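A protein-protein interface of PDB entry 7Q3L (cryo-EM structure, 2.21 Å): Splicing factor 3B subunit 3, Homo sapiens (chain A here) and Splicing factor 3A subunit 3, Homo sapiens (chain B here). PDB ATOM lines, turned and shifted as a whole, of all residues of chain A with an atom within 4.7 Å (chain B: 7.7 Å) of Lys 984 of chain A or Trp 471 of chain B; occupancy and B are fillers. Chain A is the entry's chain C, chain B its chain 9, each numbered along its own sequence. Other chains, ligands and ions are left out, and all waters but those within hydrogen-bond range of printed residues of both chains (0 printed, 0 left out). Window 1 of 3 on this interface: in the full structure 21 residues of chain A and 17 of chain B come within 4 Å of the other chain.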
ATOM      1  N   LYS A 965      22.866  17.768 -20.199  1.00  0.00           N
ATOM      2  CA  LYS A 965      21.695  16.900 -20.249  1.00  0.00           C
ATOM      3  C   LYS A 965      21.163  16.572 -18.850  1.00  0.00           C
ATOM      4  O   LYS A 965      20.212  15.795 -18.732  1.00  0.00           O
ATOM      5  CB  LYS A 965      22.018  15.601 -20.995  1.00  0.00           C
ATOM      6  CG  LYS A 965      23.077  14.721 -20.346  1.00  0.00           C
ATOM      7  CD  LYS A 965      22.699  13.260 -20.303  1.00  0.00           C
ATOM      8  CE  LYS A 965      22.475  12.644 -21.672  1.00  0.00           C
ATOM      9  NZ  LYS A 965      21.853  11.305 -21.567  1.00  0.00           N
ATOM     10  N   LEU A 966      21.781  17.137 -17.801  1.00  0.00           N
ATOM     11  CA  LEU A 966      21.409  16.814 -16.423  1.00  0.00           C
ATOM     12  C   LEU A 966      20.524  17.916 -15.843  1.00  0.00           C
ATOM     13  O   LEU A 966      20.901  19.082 -15.919  1.00  0.00           O
ATOM     14  CB  LEU A 966      22.684  16.651 -15.582  1.00  0.00           C
ATOM     15  CG  LEU A 966      23.810  15.846 -16.230  1.00  0.00           C
ATOM     16  CD1 LEU A 966      25.123  16.068 -15.497  1.00  0.00           C
ATOM     17  CD2 LEU A 966      23.466  14.364 -16.289  1.00  0.00           C
ATOM     18  N   ARG A 979      23.356  20.041  -4.263  1.00  0.00           N
ATOM     19  CA  ARG A 979      22.522  19.353  -5.244  1.00  0.00           C
ATOM     20  C   ARG A 979      21.549  18.409  -4.533  1.00  0.00           C
ATOM     21  O   ARG A 979      21.928  17.289  -4.194  1.00  0.00           O
ATOM     22  CB  ARG A 979      23.396  18.597  -6.251  1.00  0.00           C
ATOM     23  CG  ARG A 979      22.633  17.843  -7.335  1.00  0.00           C
ATOM     24  CD  ARG A 979      23.514  16.899  -8.128  1.00  0.00           C
ATOM     25  NE  ARG A 979      24.397  16.068  -7.315  1.00  0.00           N
ATOM     26  CZ  ARG A 979      25.702  16.287  -7.139  1.00  0.00           C
ATOM     27  NH1 ARG A 979      26.301  17.319  -7.713  1.00  0.00           N
ATOM     28  NH2 ARG A 979      26.404  15.472  -6.373  1.00  0.00           N
ATOM     29  N   LYS A 980      20.320  18.880  -4.283  1.00  0.00           N
ATOM     30  CA  LYS A 980      19.294  18.083  -3.623  1.00  0.00           C
ATOM     31  C   LYS A 980      18.847  16.903  -4.488  1.00  0.00           C
ATOM     32  O   LYS A 980      18.682  15.805  -3.957  1.00  0.00           O
ATOM     33  CB  LYS A 980      18.113  18.954  -3.182  1.00  0.00           C
ATOM     34  CG  LYS A 980      18.426  19.957  -2.081  1.00  0.00           C
ATOM     35  CD  LYS A 980      19.122  19.321  -0.901  1.00  0.00           C
ATOM     36  CE  LYS A 980      19.548  20.306   0.163  1.00  0.00           C
ATOM     37  NZ  LYS A 980      20.294  19.641   1.257  1.00  0.00           N
ATOM     38  N   CYS A 981      18.653  17.133  -5.796  1.00  0.00           N
ATOM     39  CA  CYS A 981      18.175  16.090  -6.707  1.00  0.00           C
ATOM     40  C   CYS A 981      18.819  16.252  -8.085  1.00  0.00           C
ATOM     41  O   CYS A 981      19.206  17.361  -8.432  1.00  0.00           O
ATOM     42  CB  CYS A 981      16.654  16.137  -6.843  1.00  0.00           C
ATOM     43  SG  CYS A 981      15.944  14.745  -7.768  1.00  0.00           S
ATOM     44  N   GLU A 982      18.930  15.154  -8.855  1.00  0.00           N
ATOM     45  CA  GLU A 982      19.432  15.216 -10.229  1.00  0.00           C
ATOM     46  C   GLU A 982      18.677  14.225 -11.121  1.00  0.00           C
ATOM     47  O   GLU A 982      18.347  13.140 -10.659  1.00  0.00           O
ATOM     48  CB  GLU A 982      20.934  14.914 -10.239  1.00  0.00           C
ATOM     49  CG  GLU A 982      21.558  14.834 -11.623  1.00  0.00           C
ATOM     50  CD  GLU A 982      23.014  14.408 -11.623  1.00  0.00           C
ATOM     51  OE1 GLU A 982      23.601  14.347 -12.717  1.00  0.00           O
ATOM     52  OE2 GLU A 982      23.562  14.133 -10.534  1.00  0.00           O
ATOM     53  N   ASN A 983      18.425  14.593 -12.390  1.00  0.00           N
ATOM     54  CA  ASN A 983      17.824  13.696 -13.373  1.00  0.00           C
ATOM     55  C   ASN A 983      18.763  13.591 -14.573  1.00  0.00           C
ATOM     56  O   ASN A 983      19.125  14.618 -15.134  1.00  0.00           O
ATOM     57  CB  ASN A 983      16.431  14.173 -13.810  1.00  0.00           C
ATOM     58  CG  ASN A 983      15.628  13.138 -14.571  1.00  0.00           C
ATOM     59  OD1 ASN A 983      14.723  13.485 -15.322  1.00  0.00           O
ATOM     60  ND2 ASN A 983      15.942  11.869 -14.373  1.00  0.00           N
ATOM     61  N   LYS A 984      19.155  12.363 -14.947  1.00  0.00           N
ATOM     62  CA  LYS A 984      20.112  12.143 -16.025  1.00  0.00           C
ATOM     63  C   LYS A 984      19.438  11.565 -17.272  1.00  0.00           C
ATOM     64  O   LYS A 984      20.136  11.189 -18.220  1.00  0.00           O
ATOM     65  CB  LYS A 984      21.236  11.208 -15.567  1.00  0.00           C
ATOM     66  CG  LYS A 984      21.803  11.508 -14.189  1.00  0.00           C
ATOM     67  CD  LYS A 984      22.780  10.464 -13.700  1.00  0.00           C
ATOM     68  CE  LYS A 984      23.363  10.791 -12.342  1.00  0.00           C
ATOM     69  NZ  LYS A 984      22.301  11.030 -11.339  1.00  0.00           N
ATOM     70  N   HIS A 985      18.095  11.510 -17.278  1.00  0.00           N
ATOM     71  CA  HIS A 985      17.369  10.838 -18.356  1.00  0.00           C
ATOM     72  C   HIS A 985      17.014  11.760 -19.528  1.00  0.00           C
ATOM     73  O   HIS A 985      16.453  11.296 -20.524  1.00  0.00           O
ATOM     74  CB  HIS A 985      16.157  10.060 -17.820  1.00  0.00           C
ATOM     75  CG  HIS A 985      16.533   8.868 -17.004  1.00  0.00           C
ATOM     76  ND1 HIS A 985      16.808   7.646 -17.576  1.00  0.00           N
ATOM     77  CD2 HIS A 985      16.689   8.710 -15.671  1.00  0.00           C
ATOM     78  CE1 HIS A 985      17.107   6.781 -16.629  1.00  0.00           C
ATOM     79  NE2 HIS A 985      17.050   7.410 -15.452  1.00  0.00           N
ATOM     80  N   ILE A 986      17.335  13.058 -19.429  1.00  0.00           N
ATOM     81  CA  ILE A 986      17.108  13.965 -20.555  1.00  0.00           C
ATOM     82  C   ILE A 986      18.006  13.526 -21.715  1.00  0.00           C
ATOM     83  O   ILE A 986      19.173  13.234 -21.495  1.00  0.00           O
ATOM     84  CB  ILE A 986      17.317  15.450 -20.174  1.00  0.00           C
ATOM     85  CG1 ILE A 986      16.362  15.914 -19.068  1.00  0.00           C
ATOM     86  CG2 ILE A 986      17.228  16.362 -21.395  1.00  0.00           C
ATOM     87  CD1 ILE A 986      16.881  15.715 -17.662  1.00  0.00           C
ATOM     88  N   ASN A1019      12.001  12.950  -3.140  1.00  0.00           N
ATOM     89  CA  ASN A1019      13.131  13.690  -3.698  1.00  0.00           C
ATOM     90  C   ASN A1019      13.566  13.204  -5.088  1.00  0.00           C
ATOM     91  O   ASN A1019      14.752  12.942  -5.318  1.00  0.00           O
ATOM     92  CB  ASN A1019      14.267  13.832  -2.681  1.00  0.00           C
ATOM     93  CG  ASN A1019      15.259  14.893  -3.099  1.00  0.00           C
ATOM     94  OD1 ASN A1019      14.897  15.869  -3.754  1.00  0.00           O
ATOM     95  ND2 ASN A1019      16.518  14.694  -2.765  1.00  0.00           N
ATOM     96  N   GLU A1068       9.939   6.078 -10.560  1.00  0.00           N
ATOM     97  CA  GLU A1068      11.150   5.537 -11.174  1.00  0.00           C
ATOM     98  C   GLU A1068      11.723   4.471 -10.237  1.00  0.00           C
ATOM     99  O   GLU A1068      11.795   4.689  -9.026  1.00  0.00           O
ATOM    100  CB  GLU A1068      12.144   6.655 -11.512  1.00  0.00           C
ATOM    101  CG  GLU A1068      13.392   6.208 -12.276  1.00  0.00           C
ATOM    102  CD  GLU A1068      14.231   7.305 -12.925  1.00  0.00           C
ATOM    103  OE1 GLU A1068      15.487   7.216 -12.878  1.00  0.00           O
ATOM    104  OE2 GLU A1068      13.639   8.241 -13.500  1.00  0.00           O
ATOM    105  N   LYS B 466      22.892   0.885 -15.627  1.00  0.00           N
ATOM    106  CA  LYS B 466      21.627   1.057 -14.913  1.00  0.00           C
ATOM    107  C   LYS B 466      21.792   1.493 -13.451  1.00  0.00           C
ATOM    108  O   LYS B 466      20.842   2.019 -12.866  1.00  0.00           O
ATOM    109  CB  LYS B 466      20.766  -0.205 -15.039  1.00  0.00           C
ATOM    110  CG  LYS B 466      20.442  -0.618 -16.471  1.00  0.00           C
ATOM    111  CD  LYS B 466      19.487   0.316 -17.177  1.00  0.00           C
ATOM    112  CE  LYS B 466      19.625   0.313 -18.684  1.00  0.00           C
ATOM    113  NZ  LYS B 466      18.813   1.399 -19.279  1.00  0.00           N
ATOM    114  N   ALA B 467      22.971   1.282 -12.847  1.00  0.00           N
ATOM    115  CA  ALA B 467      23.346   1.958 -11.607  1.00  0.00           C
ATOM    116  C   ALA B 467      23.613   3.444 -11.854  1.00  0.00           C
ATOM    117  O   ALA B 467      23.144   4.286 -11.086  1.00  0.00           O
ATOM    118  CB  ALA B 467      24.533   1.275 -10.977  1.00  0.00           C
ATOM    119  N   SER B 468      24.355   3.770 -12.929  1.00  0.00           N
ATOM    120  CA  SER B 468      24.746   5.128 -13.295  1.00  0.00           C
ATOM    121  C   SER B 468      23.554   6.013 -13.691  1.00  0.00           C
ATOM    122  O   SER B 468      23.446   7.134 -13.199  1.00  0.00           O
ATOM    123  CB  SER B 468      25.816   5.079 -14.367  1.00  0.00           C
ATOM    124  OG  SER B 468      26.255   6.370 -14.756  1.00  0.00           O
ATOM    125  N   GLU B 469      22.656   5.512 -14.557  1.00  0.00           N
ATOM    126  CA  GLU B 469      21.559   6.242 -15.198  1.00  0.00           C
ATOM    127  C   GLU B 469      20.603   6.981 -14.243  1.00  0.00           C
ATOM    128  O   GLU B 469      19.965   7.951 -14.659  1.00  0.00           O
ATOM    129  CB  GLU B 469      20.730   5.276 -16.055  1.00  0.00           C
ATOM    130  CG  GLU B 469      21.236   5.012 -17.479  1.00  0.00           C
ATOM    131  CD  GLU B 469      20.439   3.953 -18.238  1.00  0.00           C
ATOM    132  OE1 GLU B 469      19.336   3.621 -17.783  1.00  0.00           O
ATOM    133  OE2 GLU B 469      20.912   3.439 -19.273  1.00  0.00           O
ATOM    134  N   ARG B 470      20.479   6.535 -12.985  1.00  0.00           N
ATOM    135  CA  ARG B 470      19.406   6.990 -12.094  1.00  0.00           C
ATOM    136  C   ARG B 470      19.915   8.023 -11.076  1.00  0.00           C
ATOM    137  O   ARG B 470      21.073   8.431 -11.122  1.00  0.00           O
ATOM    138  CB  ARG B 470      18.728   5.758 -11.489  1.00  0.00           C
ATOM    139  CG  ARG B 470      17.995   4.958 -12.556  1.00  0.00           C
ATOM    140  CD  ARG B 470      17.339   3.690 -12.035  1.00  0.00           C
ATOM    141  NE  ARG B 470      18.366   2.724 -11.681  1.00  0.00           N
ATOM    142  CZ  ARG B 470      18.460   2.017 -10.563  1.00  0.00           C
ATOM    143  NH1 ARG B 470      17.532   2.063  -9.625  1.00  0.00           N
ATOM    144  NH2 ARG B 470      19.502   1.232 -10.390  1.00  0.00           N
ATOM    145  N   TRP B 471      19.040   8.496 -10.165  1.00  0.00           N
ATOM    146  CA  TRP B 471      19.469   9.362  -9.067  1.00  0.00           C
ATOM    147  C   TRP B 471      20.031   8.543  -7.906  1.00  0.00           C
ATOM    148  O   TRP B 471      19.377   7.618  -7.421  1.00  0.00           O
ATOM    149  CB  TRP B 471      18.338  10.299  -8.621  1.00  0.00           C
ATOM    150  CG  TRP B 471      18.584  11.193  -7.435  1.00  0.00           C
ATOM    151  CD1 TRP B 471      17.703  11.399  -6.414  1.00  0.00           C
ATOM    152  CD2 TRP B 471      19.722  12.056  -7.143  1.00  0.00           C
ATOM    153  NE1 TRP B 471      18.210  12.300  -5.514  1.00  0.00           N
ATOM    154  CE2 TRP B 471      19.451  12.731  -5.926  1.00  0.00           C
ATOM    155  CE3 TRP B 471      20.951  12.340  -7.767  1.00  0.00           C
ATOM    156  CZ2 TRP B 471      20.352  13.656  -5.357  1.00  0.00           C
ATOM    157  CZ3 TRP B 471      21.841  13.252  -7.214  1.00  0.00           C
ATOM    158  CH2 TRP B 471      21.542  13.910  -6.015  1.00  0.00           C
ATOM    159  N   GLN B 472      21.245   8.903  -7.463  1.00  0.00           N
ATOM    160  CA  GLN B 472      21.925   8.325  -6.313  1.00  0.00           C
ATOM    161  C   GLN B 472      21.758   9.266  -5.111  1.00  0.00           C
ATOM    162  O   GLN B 472      22.486  10.249  -5.005  1.00  0.00           O
ATOM    163  CB  GLN B 472      23.400   8.100  -6.680  1.00  0.00           C
ATOM    164  CG  GLN B 472      23.644   7.155  -7.862  1.00  0.00           C
ATOM    165  CD  GLN B 472      23.573   7.778  -9.241  1.00  0.00           C
ATOM    166  OE1 GLN B 472      23.557   8.996  -9.413  1.00  0.00           O
ATOM    167  NE2 GLN B 472      23.525   6.938 -10.263  1.00  0.00           N
ATOM    168  N   PRO B 473      20.783   9.041  -4.188  1.00  0.00           N
ATOM    169  CA  PRO B 473      20.546   9.953  -3.064  1.00  0.00           C
ATOM    170  C   PRO B 473      21.631   9.923  -1.979  1.00  0.00           C
ATOM    171  O   PRO B 473      21.708  10.840  -1.174  1.00  0.00           O
ATOM    172  CB  PRO B 473      19.171   9.515  -2.539  1.00  0.00           C
ATOM    173  CG  PRO B 473      19.125   8.038  -2.856  1.00  0.00           C
ATOM    174  CD  PRO B 473      19.841   7.911  -4.186  1.00  0.00           C
ATOM    175  N   ASP B 474      22.485   8.891  -1.977  1.00  0.00           N
ATOM    176  CA  ASP B 474      23.780   8.878  -1.290  1.00  0.00           C
ATOM    177  C   ASP B 474      24.730   9.988  -1.781  1.00  0.00           C
ATOM    178  O   ASP B 474      25.740  10.288  -1.144  1.00  0.00           O
ATOM    179  CB  ASP B 474      24.454   7.536  -1.567  1.00  0.00           C
ATOM    180  CG  ASP B 474      24.415   7.233  -3.054  1.00  0.00           C
ATOM    181  OD1 ASP B 474      23.382   6.710  -3.519  1.00  0.00           O
ATOM    182  OD2 ASP B 474      25.358   7.661  -3.751  1.00  0.00           O
ATOM    183  N   THR B 475      24.427  10.573  -2.950  1.00  0.00           N
ATOM    184  CA  THR B 475      25.160  11.643  -3.629  1.00  0.00           C
ATOM    185  C   THR B 475      24.319  12.932  -3.682  1.00  0.00           C
ATOM    186  O   THR B 475      24.554  13.829  -4.491  1.00  0.00           O
ATOM    187  CB  THR B 475      25.706  11.117  -4.968  1.00  0.00           C
ATOM    188  OG1 THR B 475      26.560  10.002  -4.721  1.00  0.00           O
ATOM    189  CG2 THR B 475      26.491  12.117  -5.794  1.00  0.00           C
ATOM    190  N   GLU B 476      23.331  13.050  -2.787  1.00  0.00           N
ATOM    191  CA  GLU B 476      22.735  14.322  -2.391  1.00  0.00           C
ATOM    192  C   GLU B 476      23.742  15.125  -1.556  1.00  0.00           C
ATOM    193  O   GLU B 476      24.548  14.548  -0.835  1.00  0.00           O
ATOM    194  CB  GLU B 476      21.450  14.035  -1.608  1.00  0.00           C
ATOM    195  CG  GLU B 476      20.701  15.278  -1.164  1.00  0.00           C
ATOM    196  CD  GLU B 476      19.264  15.086  -0.709  1.00  0.00           C
ATOM    197  OE1 GLU B 476      18.628  14.088  -1.115  1.00  0.00           O
ATOM    198  OE2 GLU B 476      18.764  15.962   0.012  1.00  0.00           O
ATOM    199  N   GLU B 477      23.698  16.461  -1.634  1.00  0.00           N
ATOM    200  CA  GLU B 477      24.641  17.304  -0.903  1.00  0.00           C
ATOM    201  C   GLU B 477      24.006  17.977   0.317  1.00  0.00           C
ATOM    202  O   GLU B 477      22.910  18.533   0.245  1.00  0.00           O
ATOM    203  CB  GLU B 477      25.281  18.344  -1.822  1.00  0.00           C
ATOM    204  CG  GLU B 477      25.993  17.725  -3.011  1.00  0.00           C
ATOM    205  CD  GLU B 477      26.897  18.689  -3.765  1.00  0.00           C
ATOM    206  OE1 GLU B 477      26.474  19.828  -4.029  1.00  0.00           O
ATOM    207  OE2 GLU B 477      28.038  18.297  -4.085  1.00  0.00           O
ATOM    208  N   ASN B 488      28.175  14.481   1.857  1.00  0.00           N
ATOM    209  CA  ASN B 488      27.220  13.642   1.149  1.00  0.00           C
ATOM    210  C   ASN B 488      26.969  12.426   2.056  1.00  0.00           C
ATOM    211  O   ASN B 488      27.969  11.767   2.387  1.00  0.00           O
ATOM    212  CB  ASN B 488      27.664  13.281  -0.290  1.00  0.00           C
ATOM    213  CG  ASN B 488      27.785  14.413  -1.311  1.00  0.00           C
ATOM    214  OD1 ASN B 488      27.854  14.181  -2.519  1.00  0.00           O
ATOM    215  ND2 ASN B 488      27.849  15.651  -0.854  1.00  0.00           N
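Hydrophobic or aromatic side chains of chain B that line the printed part of chain A: Trp 471. Along chain B the printed residues that touch a printed residue of chain A span positions 468 to 477. Printed residues of chain A that touch a printed residue of chain B: Arg 979, Lys 980, Cys 981, Glu 982, Lys 984, His 985, Asn 1019 and Glu 1068. Hydrophobic or aromatic side chains of chain A within 4 Å of the printed part of chain B: His 985. Among the printed residues, 19 pairs touch across the chains. Among the printed residues, Asp or Glu carboxylates within 4 Å of a Lys or Arg side-chain nitrogen of the other chain: Arg 979 of chain A with Glu 477 of chain B (3.99 Å).
The side-chain carboxylate of Glu 476 of chain B is in hydrogen-bond range of the side-chain amide nitrogen of Asn 1019 of chain A, 2.7 Å away. O of Lys 980 of chain A lies close to OE1 of Glu 476 of chain B. The guanidinium group (NH2) of Arg 979 of chain A is in salt-bridge range of the side-chain carboxylate (OE2) of Glu 477 of chain B (3.99 Å). The side-chain amino group (NZ) of Lys 984 of chain A lies within hydrogen-bond range of the side-chain amide oxygen (OE1) of Gln 472 of chain B, 3.1 Å away. The backbone carbonyl oxygen (O) of Glu 477 of chain B sits at hydrogen-bond distance from the side-chain amino group (NZ) of Lys 980 of chain A, 3.0 Å away. The guanidinium group (NH2) of Arg 979 of chain A lies within hydrogen-bond range of the backbone carbonyl oxygen (O) of Thr 475 of chain B (3.1 Å). The side-chain amino group of Lys 984 of chain A lies within hydrogen-bond range of the backbone carbonyl oxygen of Arg 470 of chain B, 2.9 Å away. NE2 of His 985 of chain A lies within hydrogen-bond range of O of Glu 469 of chain B, 3.1 Å away.
Printed residues of chain B within 4 Å of Lys 984 of chain A: Ser 468 (3.4 Å), Glu 469 (3.6 Å), Arg 470 (2.9 Å), Trp 471 (3.996 Å) and Gln 472 (3.1 Å). Printed residues of chain A within 4 Å of Ser 468 of chain B: Lys 984 (3.4 Å). Of the printed residues of chain A, Glu 469 of chain B touches Lys 984 and His 985. The nearest printed residue of chain B that does not touch Lys 984 of chain A is Ala 467 of chain B (6.6 Å). The nearest printed residue of chain A that does not touch Trp 471 of chain B is Glu 1068 of chain A (4.7 Å).
The side-chain amino group (NZ) of Lys 466 of chain B lies within salt-bridge range of the side-chain carboxylate (OE1) of Glu 469 of chain B, at 2.7 Å. SG of Cys 981 of chain A is in hydrogen-bond range of O of Asn 1019 of chain A (3.3 Å). OE2 of Glu 982 of chain A is in salt-bridge range of NE of Arg 979 of chain A, 3.8 Å away. NE of Arg 470 of chain B sits at hydrogen-bond distance from O of Lys 466 of chain B (2.8 Å). A ring nitrogen (NE2) of His 985 of chain A is in hydrogen-bond range of the side-chain carboxylate (OE1) of Glu 1068 of chain A, at 3.0 Å. The side-chain carboxylate (OE2) of Glu 982 of chain A lies within salt-bridge range of the side-chain amino group (NZ) of Lys 984 of chain A, 3.4 Å away.
Arg 979 of chain A touches Trp 471 of chain B (NE to CZ3, 3.8 Å). Arg 979 of chain A touches Glu 476 of chain B (O to CA, 3.6 Å). O of Lys 980 of chain A touches CZ2 of Trp 471 of chain B (3.1 Å). CA of Cys 981 of chain A touches CZ2 of Trp 471 of chain B, 3.5 Å away. Trp 471 of chain B touches Glu 982 of chain A (CB to O, 3.5 Å). Ser 468 of chain B touches Lys 984 of chain A. CB of Lys 984 of chain A touches O of Glu 469 of chain B (3.6 Å). Lys 984 of chain A touches Trp 471 of chain B (NZ to CA, 3.996 Å). Asn 1019 of chain A touches Trp 471 of chain B (O to CD1, 3.5 Å). Arg 470 of chain B touches Glu 1068 of chain A (CG to OE1, 3.4 Å).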
